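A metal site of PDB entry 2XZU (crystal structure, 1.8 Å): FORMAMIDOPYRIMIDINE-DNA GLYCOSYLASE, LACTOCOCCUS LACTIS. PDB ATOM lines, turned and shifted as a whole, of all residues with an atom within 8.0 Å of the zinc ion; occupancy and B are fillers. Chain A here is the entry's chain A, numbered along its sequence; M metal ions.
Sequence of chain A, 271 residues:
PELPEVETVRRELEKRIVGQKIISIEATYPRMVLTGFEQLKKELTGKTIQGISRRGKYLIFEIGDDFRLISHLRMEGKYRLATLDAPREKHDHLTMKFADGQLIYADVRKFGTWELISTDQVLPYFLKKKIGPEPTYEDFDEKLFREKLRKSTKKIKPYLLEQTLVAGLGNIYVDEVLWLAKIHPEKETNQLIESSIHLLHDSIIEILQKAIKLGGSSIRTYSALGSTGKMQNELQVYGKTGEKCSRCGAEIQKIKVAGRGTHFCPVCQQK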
ATOM      1  N   TRP A 179      -4.029 -23.477  22.989  1.00  0.00           N
ATOM      2  CA  TRP A 179      -3.634 -22.092  23.246  1.00  0.00           C
ATOM      3  C   TRP A 179      -3.527 -21.919  24.750  1.00  0.00           C
ATOM      4  O   TRP A 179      -2.568 -21.321  25.284  1.00  0.00           O
ATOM      5  CB  TRP A 179      -4.684 -21.135  22.659  1.00  0.00           C
ATOM      6  CG  TRP A 179      -4.386 -19.676  22.966  1.00  0.00           C
ATOM      7  CD1 TRP A 179      -3.628 -18.794  22.217  1.00  0.00           C
ATOM      8  CD2 TRP A 179      -4.869 -18.949  24.097  1.00  0.00           C
ATOM      9  NE1 TRP A 179      -3.625 -17.558  22.836  1.00  0.00           N
ATOM     10  CE2 TRP A 179      -4.376 -17.619  23.975  1.00  0.00           C
ATOM     11  CE3 TRP A 179      -5.667 -19.282  25.197  1.00  0.00           C
ATOM     12  CZ2 TRP A 179      -4.692 -16.608  24.913  1.00  0.00           C
ATOM     13  CZ3 TRP A 179      -5.936 -18.307  26.156  1.00  0.00           C
ATOM     14  CH2 TRP A 179      -5.451 -16.957  26.010  1.00  0.00           C
ATOM     15  N   LYS A 182      -0.390 -23.371  26.032  1.00  0.00           N
ATOM     16  CA  LYS A 182       0.822 -22.833  25.387  1.00  0.00           C
ATOM     17  C   LYS A 182       1.622 -23.912  24.658  1.00  0.00           C
ATOM     18  O   LYS A 182       2.849 -23.986  24.755  1.00  0.00           O
ATOM     19  CB  LYS A 182       1.687 -22.096  26.413  1.00  0.00           C
ATOM     20  CG  LYS A 182       1.015 -20.818  27.007  1.00  0.00           C
ATOM     21  CD  LYS A 182       1.865 -20.181  28.105  1.00  0.00           C
ATOM     22  CE  LYS A 182       1.148 -18.976  28.712  1.00  0.00           C
ATOM     23  NZ  LYS A 182       1.942 -18.147  29.712  1.00  0.00           N
ATOM     24  N   VAL A 237      -9.027 -18.318  20.376  1.00  0.00           N
ATOM     25  CA  VAL A 237      -8.371 -18.517  19.098  1.00  0.00           C
ATOM     26  C   VAL A 237      -9.256 -19.030  17.962  1.00  0.00           C
ATOM     27  O   VAL A 237      -9.059 -18.656  16.796  1.00  0.00           O
ATOM     28  CB  VAL A 237      -7.132 -19.408  19.190  1.00  0.00           C
ATOM     29  CG1 VAL A 237      -6.019 -18.694  19.943  1.00  0.00           C
ATOM     30  CG2 VAL A 237      -7.426 -20.851  19.814  1.00  0.00           C
ATOM     31  N   LYS A 244      -5.950 -10.175  17.606  1.00  0.00           N
ATOM     32  CA  LYS A 244      -4.750 -10.190  18.462  1.00  0.00           C
ATOM     33  C   LYS A 244      -4.929 -11.177  19.594  1.00  0.00           C
ATOM     34  O   LYS A 244      -6.015 -11.327  20.154  1.00  0.00           O
ATOM     35  CB  LYS A 244      -4.486  -8.796  19.021  1.00  0.00           C
ATOM     36  CG  LYS A 244      -4.346  -7.661  17.992  1.00  0.00           C
ATOM     37  CD  LYS A 244      -3.513  -7.971  16.716  1.00  0.00           C
ATOM     38  CE  LYS A 244      -3.361  -6.738  15.723  1.00  0.00           C
ATOM     39  NZ  LYS A 244      -2.299  -6.925  14.596  1.00  0.00           N
ATOM     40  N   CYS A 245      -3.878 -11.924  19.901  1.00  0.00           N
ATOM     41  CA  CYS A 245      -3.878 -12.820  21.073  1.00  0.00           C
ATOM     42  C   CYS A 245      -4.148 -12.009  22.359  1.00  0.00           C
ATOM     43  O   CYS A 245      -3.539 -10.953  22.579  1.00  0.00           O
ATOM     44  CB  CYS A 245      -2.501 -13.477  21.199  1.00  0.00           C
ATOM     45  SG  CYS A 245      -2.305 -14.483  22.678  1.00  0.00           S
ATOM     46  N   SER A 246      -5.042 -12.481  23.230  1.00  0.00           N
ATOM     47  CA  SER A 246      -5.340 -11.708  24.442  1.00  0.00           C
ATOM     48  C   SER A 246      -4.153 -11.681  25.429  1.00  0.00           C
ATOM     49  O   SER A 246      -4.096 -10.818  26.308  1.00  0.00           O
ATOM     50  CB  SER A 246      -6.581 -12.270  25.146  1.00  0.00           C
ATOM     51  OG  SER A 246      -6.311 -13.602  25.585  1.00  0.00           O
ATOM     52  N   ARG A 247      -3.217 -12.600  25.290  1.00  0.00           N
ATOM     53  CA  ARG A 247      -2.079 -12.629  26.227  1.00  0.00           C
ATOM     54  C   ARG A 247      -0.949 -11.774  25.715  1.00  0.00           C
ATOM     55  O   ARG A 247      -0.434 -10.929  26.443  1.00  0.00           O
ATOM     56  CB  ARG A 247      -1.549 -14.065  26.484  1.00  0.00           C
ATOM     57  CG  ARG A 247      -2.403 -14.825  27.467  1.00  0.00           C
ATOM     58  CD  ARG A 247      -1.789 -16.239  27.811  1.00  0.00           C
ATOM     59  NE  ARG A 247      -1.545 -16.933  26.551  1.00  0.00           N
ATOM     60  CZ  ARG A 247      -1.781 -18.222  26.355  1.00  0.00           C
ATOM     61  NH1 ARG A 247      -2.281 -18.982  27.348  1.00  0.00           N
ATOM     62  NH2 ARG A 247      -1.565 -18.754  25.166  1.00  0.00           N
ATOM     63  N   CYS A 248      -0.561 -11.940  24.458  1.00  0.00           N
ATOM     64  CA  CYS A 248       0.668 -11.243  24.008  1.00  0.00           C
ATOM     65  C   CYS A 248       0.488 -10.220  22.909  1.00  0.00           C
ATOM     66  O   CYS A 248       1.434  -9.476  22.642  1.00  0.00           O
ATOM     67  CB  CYS A 248       1.696 -12.259  23.545  1.00  0.00           C
ATOM     68  SG  CYS A 248       1.221 -12.964  22.038  1.00  0.00           S
ATOM     69  N   GLY A 249      -0.679 -10.158  22.268  1.00  0.00           N
ATOM     70  CA  GLY A 249      -0.924  -9.136  21.246  1.00  0.00           C
ATOM     71  C   GLY A 249      -0.501  -9.563  19.846  1.00  0.00           C
ATOM     72  O   GLY A 249      -0.756  -8.847  18.867  1.00  0.00           O
ATOM     73  N   ALA A 250       0.105 -10.739  19.707  1.00  0.00           N
ATOM     74  CA  ALA A 250       0.427 -11.213  18.359  1.00  0.00           C
ATOM     75  C   ALA A 250      -0.858 -11.526  17.588  1.00  0.00           C
ATOM     76  O   ALA A 250      -1.795 -11.992  18.228  1.00  0.00           O
ATOM     77  CB  ALA A 250       1.322 -12.424  18.408  1.00  0.00           C
ATOM     78  N   GLU A 251      -0.897 -11.379  16.258  1.00  0.00           N
ATOM     79  CA  GLU A 251      -2.048 -11.937  15.474  1.00  0.00           C
ATOM     80  C   GLU A 251      -2.184 -13.449  15.529  1.00  0.00           C
ATOM     81  O   GLU A 251      -1.218 -14.216  15.351  1.00  0.00           O
ATOM     82  CB  GLU A 251      -2.112 -11.530  13.982  1.00  0.00           C
ATOM     83  CG  GLU A 251      -1.986 -10.132  13.771  1.00  0.00           C
ATOM     84  CD  GLU A 251      -2.547  -9.669  12.431  1.00  0.00           C
ATOM     85  OE1 GLU A 251      -2.761 -10.458  11.477  1.00  0.00           O
ATOM     86  OE2 GLU A 251      -2.807  -8.518  12.372  1.00  0.00           O
ATOM     87  N   ILE A 252      -3.411 -13.886  15.761  1.00  0.00           N
ATOM     88  CA  ILE A 252      -3.701 -15.320  15.663  1.00  0.00           C
ATOM     89  C   ILE A 252      -3.586 -15.759  14.216  1.00  0.00           C
ATOM     90  O   ILE A 252      -4.070 -15.064  13.276  1.00  0.00           O
ATOM     91  CB  ILE A 252      -5.148 -15.585  16.144  1.00  0.00           C
ATOM     92  CG1 ILE A 252      -5.303 -15.133  17.608  1.00  0.00           C
ATOM     93  CG2 ILE A 252      -5.556 -17.063  15.932  1.00  0.00           C
ATOM     94  CD1 ILE A 252      -4.182 -15.685  18.575  1.00  0.00           C
ATOM     95  N   PHE A 264      -3.924 -20.577  16.133  1.00  0.00           N
ATOM     96  CA  PHE A 264      -3.006 -20.596  17.291  1.00  0.00           C
ATOM     97  C   PHE A 264      -2.294 -19.248  17.353  1.00  0.00           C
ATOM     98  O   PHE A 264      -2.284 -18.472  16.387  1.00  0.00           O
ATOM     99  CB  PHE A 264      -1.989 -21.756  17.130  1.00  0.00           C
ATOM    100  CG  PHE A 264      -0.989 -21.506  16.011  1.00  0.00           C
ATOM    101  CD1 PHE A 264      -1.363 -21.646  14.666  1.00  0.00           C
ATOM    102  CD2 PHE A 264       0.318 -21.069  16.302  1.00  0.00           C
ATOM    103  CE1 PHE A 264      -0.481 -21.337  13.607  1.00  0.00           C
ATOM    104  CE2 PHE A 264       1.225 -20.796  15.257  1.00  0.00           C
ATOM    105  CZ  PHE A 264       0.822 -20.912  13.910  1.00  0.00           C
ATOM    106  N   CYS A 265      -1.663 -18.961  18.498  1.00  0.00           N
ATOM    107  CA  CYS A 265      -0.829 -17.788  18.605  1.00  0.00           C
ATOM    108  C   CYS A 265       0.642 -18.229  18.440  1.00  0.00           C
ATOM    109  O   CYS A 265       1.095 -19.029  19.219  1.00  0.00           O
ATOM    110  CB  CYS A 265      -0.948 -17.149  20.016  1.00  0.00           C
ATOM    111  SG  CYS A 265       0.250 -15.786  20.356  1.00  0.00           S
ATOM    112  N   PRO A 266       1.360 -17.716  17.429  1.00  0.00           N
ATOM    113  CA  PRO A 266       2.730 -18.128  17.181  1.00  0.00           C
ATOM    114  C   PRO A 266       3.708 -17.699  18.265  1.00  0.00           C
ATOM    115  O   PRO A 266       4.822 -18.204  18.221  1.00  0.00           O
ATOM    116  CB  PRO A 266       3.129 -17.395  15.868  1.00  0.00           C
ATOM    117  CG  PRO A 266       1.861 -16.788  15.372  1.00  0.00           C
ATOM    118  CD  PRO A 266       0.921 -16.673  16.486  1.00  0.00           C
ATOM    119  N   VAL A 267       3.365 -16.761  19.135  1.00  0.00           N
ATOM    120  CA  VAL A 267       4.306 -16.367  20.247  1.00  0.00           C
ATOM    121  C   VAL A 267       4.089 -17.324  21.421  1.00  0.00           C
ATOM    122  O   VAL A 267       5.021 -17.886  22.012  1.00  0.00           O
ATOM    123  CB  VAL A 267       4.025 -14.904  20.705  1.00  0.00           C
ATOM    124  CG1 VAL A 267       4.827 -14.577  21.986  1.00  0.00           C
ATOM    125  CG2 VAL A 267       4.513 -13.937  19.612  1.00  0.00           C
ATOM    126  N   CYS A 268       2.829 -17.459  21.806  1.00  0.00           N
ATOM    127  CA  CYS A 268       2.466 -18.234  22.994  1.00  0.00           C
ATOM    128  C   CYS A 268       2.605 -19.742  22.754  1.00  0.00           C
ATOM    129  O   CYS A 268       2.750 -20.497  23.722  1.00  0.00           O
ATOM    130  CB  CYS A 268       0.982 -17.968  23.366  1.00  0.00           C
ATOM    131  SG  CYS A 268       0.714 -16.293  24.088  1.00  0.00           S
ATOM    132  N   GLN A 269       2.498 -20.173  21.498  1.00  0.00           N
ATOM    133  CA  GLN A 269       2.555 -21.601  21.157  1.00  0.00           C
ATOM    134  C   GLN A 269       3.760 -21.811  20.247  1.00  0.00           C
ATOM    135  O   GLN A 269       3.667 -21.814  19.041  1.00  0.00           O
ATOM    136  CB  GLN A 269       1.223 -22.104  20.525  1.00  0.00           C
ATOM    137  CG  GLN A 269       0.052 -21.816  21.468  1.00  0.00           C
ATOM    138  CD  GLN A 269      -1.277 -21.980  20.714  1.00  0.00           C
ATOM    139  OE1 GLN A 269      -1.880 -20.978  20.353  1.00  0.00           O
ATOM    140  NE2 GLN A 269      -1.707 -23.227  20.458  1.00  0.00           N
HETATM  141 ZN    ZN M   1      -0.023 -14.924  22.341  1.00  0.00          ZN
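SG of Cys 265 lies close to N of Val 267 (3.5 Å). OE1 of Gln 269 sits at hydrogen-bond distance from N of Cys 265, 2.7 Å away. The side-chain sulfur (SG) of Cys 268 lies close to the guanidinium group (NE) of Arg 247, 3.4 Å away. SG of Cys 248 sits close to N of Ala 250 (3.4 Å). The indole nitrogen (NE1) of Trp 179 sits close to the side-chain sulfur (SG) of Cys 245, at 3.4 Å. The side-chain sulfur of Cys 245 sits close to the backbone NH of Arg 247 (3.3 Å). O of Ala 250 is in hydrogen-bond range of N of Cys 245, 2.7 Å away.
The zinc ion is bound by the side-chain sulfur of Cys 265 (2.2 Å), the side-chain sulfur of Cys 268 (2.3 Å), the side-chain sulfur of Cys 248 (2.3 Å) and the side-chain sulfur of Cys 245 (2.3 Å). The zinc ion has four donor atoms within binding distance.
Of the 18 residues printed, 4 come within 4 Å of the zinc ion. The nearest printed residue that does not touch the zinc ion is Val 267 (4.4 Å).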
